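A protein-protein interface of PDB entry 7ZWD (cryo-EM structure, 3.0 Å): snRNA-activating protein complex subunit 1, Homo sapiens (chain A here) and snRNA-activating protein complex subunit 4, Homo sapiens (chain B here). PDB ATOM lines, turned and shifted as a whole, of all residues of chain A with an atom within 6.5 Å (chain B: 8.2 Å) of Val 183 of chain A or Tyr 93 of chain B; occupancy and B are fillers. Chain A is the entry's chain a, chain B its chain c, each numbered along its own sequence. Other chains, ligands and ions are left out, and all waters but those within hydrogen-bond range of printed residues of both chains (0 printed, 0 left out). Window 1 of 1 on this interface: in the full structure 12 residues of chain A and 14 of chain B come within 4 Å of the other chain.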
ATOM      1  N   GLU A 178       3.023  23.872 -13.158  1.00  0.00           N
ATOM      2  CA  GLU A 178       2.447  24.956 -13.948  1.00  0.00           C
ATOM      3  C   GLU A 178       3.532  25.873 -14.496  1.00  0.00           C
ATOM      4  O   GLU A 178       3.550  26.176 -15.695  1.00  0.00           O
ATOM      5  CB  GLU A 178       1.445  25.748 -13.108  1.00  0.00           C
ATOM      6  CG  GLU A 178       0.061  25.112 -12.998  1.00  0.00           C
ATOM      7  CD  GLU A 178      -0.420  24.482 -14.296  1.00  0.00           C
ATOM      8  OE1 GLU A 178      -0.283  25.116 -15.364  1.00  0.00           O
ATOM      9  OE2 GLU A 178      -0.936  23.346 -14.247  1.00  0.00           O
ATOM     10  N   GLU A 179       4.447  26.325 -13.635  1.00  0.00           N
ATOM     11  CA  GLU A 179       5.560  27.143 -14.108  1.00  0.00           C
ATOM     12  C   GLU A 179       6.441  26.366 -15.078  1.00  0.00           C
ATOM     13  O   GLU A 179       6.981  26.941 -16.031  1.00  0.00           O
ATOM     14  CB  GLU A 179       6.386  27.658 -12.930  1.00  0.00           C
ATOM     15  CG  GLU A 179       5.583  28.370 -11.853  1.00  0.00           C
ATOM     16  CD  GLU A 179       6.138  28.128 -10.464  1.00  0.00           C
ATOM     17  OE1 GLU A 179       5.577  28.676  -9.492  1.00  0.00           O
ATOM     18  OE2 GLU A 179       7.135  27.387 -10.344  1.00  0.00           O
ATOM     19  N   MET A 180       6.589  25.058 -14.860  1.00  0.00           N
ATOM     20  CA  MET A 180       7.385  24.242 -15.771  1.00  0.00           C
ATOM     21  C   MET A 180       6.783  24.246 -17.171  1.00  0.00           C
ATOM     22  O   MET A 180       7.486  24.474 -18.160  1.00  0.00           O
ATOM     23  CB  MET A 180       7.506  22.816 -15.224  1.00  0.00           C
ATOM     24  CG  MET A 180       8.211  21.812 -16.140  1.00  0.00           C
ATOM     25  SD  MET A 180       7.201  21.068 -17.441  1.00  0.00           S
ATOM     26  CE  MET A 180       5.706  20.676 -16.537  1.00  0.00           C
ATOM     27  N   LEU A 181       5.472  24.011 -17.271  1.00  0.00           N
ATOM     28  CA  LEU A 181       4.841  23.967 -18.587  1.00  0.00           C
ATOM     29  C   LEU A 181       4.765  25.355 -19.212  1.00  0.00           C
ATOM     30  O   LEU A 181       4.832  25.491 -20.438  1.00  0.00           O
ATOM     31  CB  LEU A 181       3.454  23.324 -18.493  1.00  0.00           C
ATOM     32  CG  LEU A 181       2.340  23.972 -17.672  1.00  0.00           C
ATOM     33  CD1 LEU A 181       1.442  24.825 -18.557  1.00  0.00           C
ATOM     34  CD2 LEU A 181       1.524  22.910 -16.953  1.00  0.00           C
ATOM     35  N   ASN A 182       4.652  26.401 -18.386  1.00  0.00           N
ATOM     36  CA  ASN A 182       4.725  27.762 -18.913  1.00  0.00           C
ATOM     37  C   ASN A 182       6.086  28.032 -19.541  1.00  0.00           C
ATOM     38  O   ASN A 182       6.176  28.535 -20.668  1.00  0.00           O
ATOM     39  CB  ASN A 182       4.433  28.779 -17.807  1.00  0.00           C
ATOM     40  CG  ASN A 182       3.032  28.652 -17.247  1.00  0.00           C
ATOM     41  OD1 ASN A 182       2.282  27.749 -17.614  1.00  0.00           O
ATOM     42  ND2 ASN A 182       2.671  29.560 -16.347  1.00  0.00           N
ATOM     43  N   VAL A 183       7.164  27.711 -18.823  1.00  0.00           N
ATOM     44  CA  VAL A 183       8.492  27.923 -19.383  1.00  0.00           C
ATOM     45  C   VAL A 183       8.694  27.059 -20.622  1.00  0.00           C
ATOM     46  O   VAL A 183       9.301  27.504 -21.600  1.00  0.00           O
ATOM     47  CB  VAL A 183       9.577  27.662 -18.322  1.00  0.00           C
ATOM     48  CG1 VAL A 183      10.958  27.801 -18.935  1.00  0.00           C
ATOM     49  CG2 VAL A 183       9.420  28.628 -17.159  1.00  0.00           C
ATOM     50  N   HIS A 184       8.147  25.840 -20.628  1.00  0.00           N
ATOM     51  CA  HIS A 184       8.310  24.957 -21.780  1.00  0.00           C
ATOM     52  C   HIS A 184       7.602  25.505 -23.017  1.00  0.00           C
ATOM     53  O   HIS A 184       8.183  25.544 -24.110  1.00  0.00           O
ATOM     54  CB  HIS A 184       7.804  23.554 -21.442  1.00  0.00           C
ATOM     55  CG  HIS A 184       8.800  22.716 -20.702  1.00  0.00           C
ATOM     56  ND1 HIS A 184       9.061  21.405 -21.034  1.00  0.00           N
ATOM     57  CD2 HIS A 184       9.609  23.007 -19.655  1.00  0.00           C
ATOM     58  CE1 HIS A 184       9.982  20.920 -20.220  1.00  0.00           C
ATOM     59  NE2 HIS A 184      10.331  21.872 -19.373  1.00  0.00           N
ATOM     60  N   ASP A 185       6.341  25.925 -22.877  1.00  0.00           N
ATOM     61  CA  ASP A 185       5.632  26.401 -24.061  1.00  0.00           C
ATOM     62  C   ASP A 185       6.145  27.766 -24.508  1.00  0.00           C
ATOM     63  O   ASP A 185       6.159  28.051 -25.710  1.00  0.00           O
ATOM     64  CB  ASP A 185       4.112  26.402 -23.826  1.00  0.00           C
ATOM     65  CG  ASP A 185       3.594  27.662 -23.139  1.00  0.00           C
ATOM     66  OD1 ASP A 185       2.372  27.904 -23.230  1.00  0.00           O
ATOM     67  OD2 ASP A 185       4.363  28.395 -22.492  1.00  0.00           O
ATOM     68  N   HIS A 186       6.604  28.606 -23.574  1.00  0.00           N
ATOM     69  CA  HIS A 186       7.282  29.837 -23.970  1.00  0.00           C
ATOM     70  C   HIS A 186       8.571  29.521 -24.719  1.00  0.00           C
ATOM     71  O   HIS A 186       8.926  30.198 -25.692  1.00  0.00           O
ATOM     72  CB  HIS A 186       7.558  30.697 -22.734  1.00  0.00           C
ATOM     73  CG  HIS A 186       8.154  32.037 -23.042  1.00  0.00           C
ATOM     74  ND1 HIS A 186       9.411  32.190 -23.586  1.00  0.00           N
ATOM     75  CD2 HIS A 186       7.661  33.288 -22.880  1.00  0.00           C
ATOM     76  CE1 HIS A 186       9.668  33.476 -23.745  1.00  0.00           C
ATOM     77  NE2 HIS A 186       8.622  34.164 -23.325  1.00  0.00           N
ATOM     78  N   TYR A 187       9.272  28.470 -24.285  1.00  0.00           N
ATOM     79  CA  TYR A 187      10.479  28.024 -24.967  1.00  0.00           C
ATOM     80  C   TYR A 187      10.169  27.587 -26.392  1.00  0.00           C
ATOM     81  O   TYR A 187      10.908  27.912 -27.326  1.00  0.00           O
ATOM     82  CB  TYR A 187      11.112  26.886 -24.164  1.00  0.00           C
ATOM     83  CG  TYR A 187      12.518  26.520 -24.563  1.00  0.00           C
ATOM     84  CD1 TYR A 187      13.484  27.498 -24.746  1.00  0.00           C
ATOM     85  CD2 TYR A 187      12.889  25.193 -24.723  1.00  0.00           C
ATOM     86  CE1 TYR A 187      14.775  27.166 -25.101  1.00  0.00           C
ATOM     87  CE2 TYR A 187      14.177  24.849 -25.077  1.00  0.00           C
ATOM     88  CZ  TYR A 187      15.115  25.840 -25.267  1.00  0.00           C
ATOM     89  OH  TYR A 187      16.404  25.509 -25.618  1.00  0.00           O
ATOM     90  N   GLN A 188       9.059  26.873 -26.580  1.00  0.00           N
ATOM     91  CA  GLN A 188       8.652  26.479 -27.927  1.00  0.00           C
ATOM     92  C   GLN A 188       8.289  27.695 -28.777  1.00  0.00           C
ATOM     93  O   GLN A 188       8.668  27.787 -29.953  1.00  0.00           O
ATOM     94  CB  GLN A 188       7.478  25.498 -27.861  1.00  0.00           C
ATOM     95  CG  GLN A 188       7.663  24.301 -26.927  1.00  0.00           C
ATOM     96  CD  GLN A 188       9.102  23.810 -26.821  1.00  0.00           C
ATOM     97  OE1 GLN A 188       9.803  23.661 -27.824  1.00  0.00           O
ATOM     98  NE2 GLN A 188       9.546  23.556 -25.595  1.00  0.00           N
ATOM     99  N   ILE A 208      14.737  19.138 -27.407  1.00  0.00           N
ATOM    100  CA  ILE A 208      13.869  19.361 -26.259  1.00  0.00           C
ATOM    101  C   ILE A 208      12.921  18.176 -26.101  1.00  0.00           C
ATOM    102  O   ILE A 208      12.404  17.620 -27.081  1.00  0.00           O
ATOM    103  CB  ILE A 208      13.099  20.688 -26.399  1.00  0.00           C
ATOM    104  CG1 ILE A 208      12.321  21.000 -25.118  1.00  0.00           C
ATOM    105  CG2 ILE A 208      12.174  20.662 -27.610  1.00  0.00           C
ATOM    106  CD1 ILE A 208      13.166  20.979 -23.863  1.00  0.00           C
ATOM    107  N   PHE A 212       8.950  15.118 -20.299  1.00  0.00           N
ATOM    108  CA  PHE A 212       9.334  15.512 -18.946  1.00  0.00           C
ATOM    109  C   PHE A 212       8.115  15.600 -18.039  1.00  0.00           C
ATOM    110  O   PHE A 212       8.106  15.047 -16.932  1.00  0.00           O
ATOM    111  CB  PHE A 212      10.074  16.848 -18.977  1.00  0.00           C
ATOM    112  CG  PHE A 212      10.511  17.324 -17.622  1.00  0.00           C
ATOM    113  CD1 PHE A 212      11.599  16.748 -16.991  1.00  0.00           C
ATOM    114  CD2 PHE A 212       9.830  18.342 -16.977  1.00  0.00           C
ATOM    115  CE1 PHE A 212      12.004  17.179 -15.743  1.00  0.00           C
ATOM    116  CE2 PHE A 212      10.231  18.780 -15.728  1.00  0.00           C
ATOM    117  CZ  PHE A 212      11.321  18.197 -15.111  1.00  0.00           C
ATOM    118  N   CYS B  86      17.790  33.070 -27.228  1.00  0.00           N
ATOM    119  CA  CYS B  86      17.795  31.637 -26.957  1.00  0.00           C
ATOM    120  C   CYS B  86      18.794  31.300 -25.862  1.00  0.00           C
ATOM    121  O   CYS B  86      18.466  30.566 -24.921  1.00  0.00           O
ATOM    122  CB  CYS B  86      18.112  30.856 -28.231  1.00  0.00           C
ATOM    123  SG  CYS B  86      17.514  29.151 -28.229  1.00  0.00           S
ATOM    124  N   LEU B  87      20.010  31.845 -25.962  1.00  0.00           N
ATOM    125  CA  LEU B  87      21.002  31.632 -24.916  1.00  0.00           C
ATOM    126  C   LEU B  87      20.468  32.061 -23.560  1.00  0.00           C
ATOM    127  O   LEU B  87      20.520  31.289 -22.600  1.00  0.00           O
ATOM    128  CB  LEU B  87      22.295  32.391 -25.218  1.00  0.00           C
ATOM    129  CG  LEU B  87      22.921  32.451 -26.606  1.00  0.00           C
ATOM    130  CD1 LEU B  87      24.204  33.242 -26.520  1.00  0.00           C
ATOM    131  CD2 LEU B  87      23.201  31.056 -27.111  1.00  0.00           C
ATOM    132  N   GLN B  88      19.940  33.284 -23.460  1.00  0.00           N
ATOM    133  CA  GLN B  88      19.589  33.797 -22.137  1.00  0.00           C
ATOM    134  C   GLN B  88      18.404  33.040 -21.535  1.00  0.00           C
ATOM    135  O   GLN B  88      18.394  32.746 -20.331  1.00  0.00           O
ATOM    136  CB  GLN B  88      19.318  35.306 -22.187  1.00  0.00           C
ATOM    137  CG  GLN B  88      18.255  35.780 -23.163  1.00  0.00           C
ATOM    138  CD  GLN B  88      16.839  35.623 -22.637  1.00  0.00           C
ATOM    139  OE1 GLN B  88      16.620  35.504 -21.431  1.00  0.00           O
ATOM    140  NE2 GLN B  88      15.869  35.624 -23.544  1.00  0.00           N
ATOM    141  N   LEU B  89      17.406  32.685 -22.355  1.00  0.00           N
ATOM    142  CA  LEU B  89      16.256  31.981 -21.797  1.00  0.00           C
ATOM    143  C   LEU B  89      16.615  30.542 -21.444  1.00  0.00           C
ATOM    144  O   LEU B  89      16.165  30.016 -20.417  1.00  0.00           O
ATOM    145  CB  LEU B  89      15.069  32.032 -22.762  1.00  0.00           C
ATOM    146  CG  LEU B  89      13.859  31.163 -22.388  1.00  0.00           C
ATOM    147  CD1 LEU B  89      13.399  31.472 -20.970  1.00  0.00           C
ATOM    148  CD2 LEU B  89      12.705  31.366 -23.350  1.00  0.00           C
ATOM    149  N   ASN B  90      17.445  29.887 -22.261  1.00  0.00           N
ATOM    150  CA  ASN B  90      17.897  28.553 -21.890  1.00  0.00           C
ATOM    151  C   ASN B  90      18.763  28.602 -20.638  1.00  0.00           C
ATOM    152  O   ASN B  90      18.726  27.681 -19.819  1.00  0.00           O
ATOM    153  CB  ASN B  90      18.644  27.898 -23.051  1.00  0.00           C
ATOM    154  CG  ASN B  90      18.385  26.406 -23.132  1.00  0.00           C
ATOM    155  OD1 ASN B  90      17.238  25.969 -23.204  1.00  0.00           O
ATOM    156  ND2 ASN B  90      19.451  25.617 -23.120  1.00  0.00           N
ATOM    157  N   MET B  91      19.525  29.685 -20.454  1.00  0.00           N
ATOM    158  CA  MET B  91      20.321  29.828 -19.238  1.00  0.00           C
ATOM    159  C   MET B  91      19.443  30.001 -18.006  1.00  0.00           C
ATOM    160  O   MET B  91      19.728  29.416 -16.957  1.00  0.00           O
ATOM    161  CB  MET B  91      21.299  31.002 -19.361  1.00  0.00           C
ATOM    162  CG  MET B  91      22.448  30.810 -20.352  1.00  0.00           C
ATOM    163  SD  MET B  91      23.477  29.337 -20.136  1.00  0.00           S
ATOM    164  CE  MET B  91      23.636  29.240 -18.351  1.00  0.00           C
ATOM    165  N   VAL B  92      18.374  30.797 -18.096  1.00  0.00           N
ATOM    166  CA  VAL B  92      17.523  30.962 -16.916  1.00  0.00           C
ATOM    167  C   VAL B  92      16.733  29.681 -16.645  1.00  0.00           C
ATOM    168  O   VAL B  92      16.430  29.353 -15.488  1.00  0.00           O
ATOM    169  CB  VAL B  92      16.608  32.197 -17.054  1.00  0.00           C
ATOM    170  CG1 VAL B  92      15.690  32.081 -18.245  1.00  0.00           C
ATOM    171  CG2 VAL B  92      15.811  32.425 -15.772  1.00  0.00           C
ATOM    172  N   TYR B  93      16.416  28.916 -17.696  1.00  0.00           N
ATOM    173  CA  TYR B  93      15.796  27.613 -17.471  1.00  0.00           C
ATOM    174  C   TYR B  93      16.770  26.634 -16.818  1.00  0.00           C
ATOM    175  O   TYR B  93      16.382  25.888 -15.906  1.00  0.00           O
ATOM    176  CB  TYR B  93      15.246  27.051 -18.784  1.00  0.00           C
ATOM    177  CG  TYR B  93      14.527  25.727 -18.635  1.00  0.00           C
ATOM    178  CD1 TYR B  93      13.386  25.618 -17.850  1.00  0.00           C
ATOM    179  CD2 TYR B  93      14.969  24.595 -19.305  1.00  0.00           C
ATOM    180  CE1 TYR B  93      12.722  24.415 -17.716  1.00  0.00           C
ATOM    181  CE2 TYR B  93      14.310  23.387 -19.179  1.00  0.00           C
ATOM    182  CZ  TYR B  93      13.187  23.302 -18.384  1.00  0.00           C
ATOM    183  OH  TYR B  93      12.528  22.102 -18.257  1.00  0.00           O
ATOM    184  N   GLN B  94      18.034  26.627 -17.256  1.00  0.00           N
ATOM    185  CA  GLN B  94      19.064  25.884 -16.536  1.00  0.00           C
ATOM    186  C   GLN B  94      19.172  26.354 -15.094  1.00  0.00           C
ATOM    187  O   GLN B  94      19.400  25.545 -14.194  1.00  0.00           O
ATOM    188  CB  GLN B  94      20.415  25.977 -17.252  1.00  0.00           C
ATOM    189  CG  GLN B  94      20.436  25.506 -18.693  1.00  0.00           C
ATOM    190  CD  GLN B  94      21.794  24.962 -19.098  1.00  0.00           C
ATOM    191  OE1 GLN B  94      21.886  23.941 -19.781  1.00  0.00           O
ATOM    192  NE2 GLN B  94      22.854  25.637 -18.675  1.00  0.00           N
ATOM    193  N   GLU B  95      18.995  27.653 -14.855  1.00  0.00           N
ATOM    194  CA  GLU B  95      19.114  28.182 -13.500  1.00  0.00           C
ATOM    195  C   GLU B  95      18.000  27.654 -12.604  1.00  0.00           C
ATOM    196  O   GLU B  95      18.252  27.240 -11.465  1.00  0.00           O
ATOM    197  CB  GLU B  95      19.116  29.714 -13.542  1.00  0.00           C
ATOM    198  CG  GLU B  95      19.069  30.424 -12.187  1.00  0.00           C
ATOM    199  CD  GLU B  95      17.669  30.539 -11.613  1.00  0.00           C
ATOM    200  OE1 GLU B  95      17.472  30.168 -10.437  1.00  0.00           O
ATOM    201  OE2 GLU B  95      16.766  31.005 -12.339  1.00  0.00           O
ATOM    202  N   VAL B  96      16.761  27.656 -13.098  1.00  0.00           N
ATOM    203  CA  VAL B  96      15.652  27.192 -12.265  1.00  0.00           C
ATOM    204  C   VAL B  96      15.736  25.681 -12.057  1.00  0.00           C
ATOM    205  O   VAL B  96      15.502  25.175 -10.950  1.00  0.00           O
ATOM    206  CB  VAL B  96      14.295  27.624 -12.856  1.00  0.00           C
ATOM    207  CG1 VAL B  96      14.124  27.141 -14.280  1.00  0.00           C
ATOM    208  CG2 VAL B  96      13.149  27.131 -11.978  1.00  0.00           C
ATOM    209  N   ILE B  97      16.120  24.934 -13.100  1.00  0.00           N
ATOM    210  CA  ILE B  97      16.238  23.491 -12.901  1.00  0.00           C
ATOM    211  C   ILE B  97      17.460  23.167 -12.046  1.00  0.00           C
ATOM    212  O   ILE B  97      17.495  22.132 -11.374  1.00  0.00           O
ATOM    213  CB  ILE B  97      16.268  22.739 -14.245  1.00  0.00           C
ATOM    214  CG1 ILE B  97      16.246  21.228 -14.001  1.00  0.00           C
ATOM    215  CG2 ILE B  97      17.512  23.086 -15.025  1.00  0.00           C
ATOM    216  CD1 ILE B  97      16.129  20.408 -15.249  1.00  0.00           C
ATOM    217  N   GLN B  98      18.458  24.053 -12.011  1.00  0.00           N
ATOM    218  CA  GLN B  98      19.615  23.832 -11.152  1.00  0.00           C
ATOM    219  C   GLN B  98      19.274  24.119  -9.697  1.00  0.00           C
ATOM    220  O   GLN B  98      19.758  23.430  -8.793  1.00  0.00           O
ATOM    221  CB  GLN B  98      20.783  24.705 -11.619  1.00  0.00           C
ATOM    222  CG  GLN B  98      22.043  24.639 -10.755  1.00  0.00           C
ATOM    223  CD  GLN B  98      22.381  23.235 -10.283  1.00  0.00           C
ATOM    224  OE1 GLN B  98      22.314  22.273 -11.050  1.00  0.00           O
ATOM    225  NE2 GLN B  98      22.746  23.111  -9.012  1.00  0.00           N
ATOM    226  N   GLU B  99      18.447  25.137  -9.451  1.00  0.00           N
ATOM    227  CA  GLU B  99      17.896  25.319  -8.112  1.00  0.00           C
ATOM    228  C   GLU B  99      17.107  24.084  -7.692  1.00  0.00           C
ATOM    229  O   GLU B  99      17.230  23.609  -6.554  1.00  0.00           O
ATOM    230  CB  GLU B  99      17.018  26.574  -8.071  1.00  0.00           C
ATOM    231  CG  GLU B  99      16.661  27.094  -6.671  1.00  0.00           C
ATOM    232  CD  GLU B  99      15.719  26.182  -5.904  1.00  0.00           C
ATOM    233  OE1 GLU B  99      14.671  25.799  -6.463  1.00  0.00           O
ATOM    234  OE2 GLU B  99      16.028  25.846  -4.742  1.00  0.00           O
ATOM    235  N   LYS B 100      16.297  23.545  -8.608  1.00  0.00           N
ATOM    236  CA  LYS B 100      15.543  22.332  -8.307  1.00  0.00           C
ATOM    237  C   LYS B 100      16.472  21.161  -7.997  1.00  0.00           C
ATOM    238  O   LYS B 100      16.219  20.391  -7.063  1.00  0.00           O
ATOM    239  CB  LYS B 100      14.624  21.989  -9.476  1.00  0.00           C
ATOM    240  CG  LYS B 100      13.398  21.202  -9.071  1.00  0.00           C
ATOM    241  CD  LYS B 100      12.242  22.136  -8.773  1.00  0.00           C
ATOM    242  CE  LYS B 100      11.121  21.403  -8.075  1.00  0.00           C
ATOM    243  NZ  LYS B 100      10.474  20.400  -8.960  1.00  0.00           N
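NE2 of His 184 of chain A lies within hydrogen-bond range of SD of Met 180 of chain A, at 3.8 Å. The backbone carbonyl oxygen (O) of His 184 of chain A sits at hydrogen-bond distance from the side-chain amide nitrogen (NE2) of Gln 188 of chain A, at 2.8 Å.
Val 183 of chain A touches just one residue of chain B: Tyr 93 (3.4 Å). Printed residues of chain B within 4 Å of His 184 of chain A: Tyr 93 (2.5 Å). Asp 185 of chain A touches none of the printed residues of chain B. Of the printed residues of chain A, Asn 90 of chain B touches Tyr 187. Of the printed residues of chain A, Tyr 93 of chain B touches Val 183 and His 184. Glu 99 of chain B touches none of the printed residues of chain A.
The side-chain hydroxyl of Tyr 187 of chain A lies within hydrogen-bond range of the side-chain amide oxygen of Asn 90 of chain B. The side-chain hydroxyl of Tyr 93 of chain B lies within hydrogen-bond range of a ring nitrogen (NE2) of His 184 of chain A, at 2.5 Å.
Tyr 93 of chain B touches Val 183 of chain A. CD2 of Leu 89 of chain B touches ND1 of His 186 of chain A, at 3.4 Å.
Printed residues of chain A that touch a printed residue of chain B: Val 183, His 184, His 186 and Tyr 187. Hydrophobic or aromatic side chains of chain A within 4 Å of the printed part of chain B: Val 183, His 184, His 186 and Tyr 187. Along chain A the printed residues that touch a printed residue of chain B span positions 183 to 187. Hydrophobic or aromatic side chains of chain B that line the printed part of chain A: Leu 89 and Tyr 93. Among the printed residues, 4 pairs touch across the chains.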
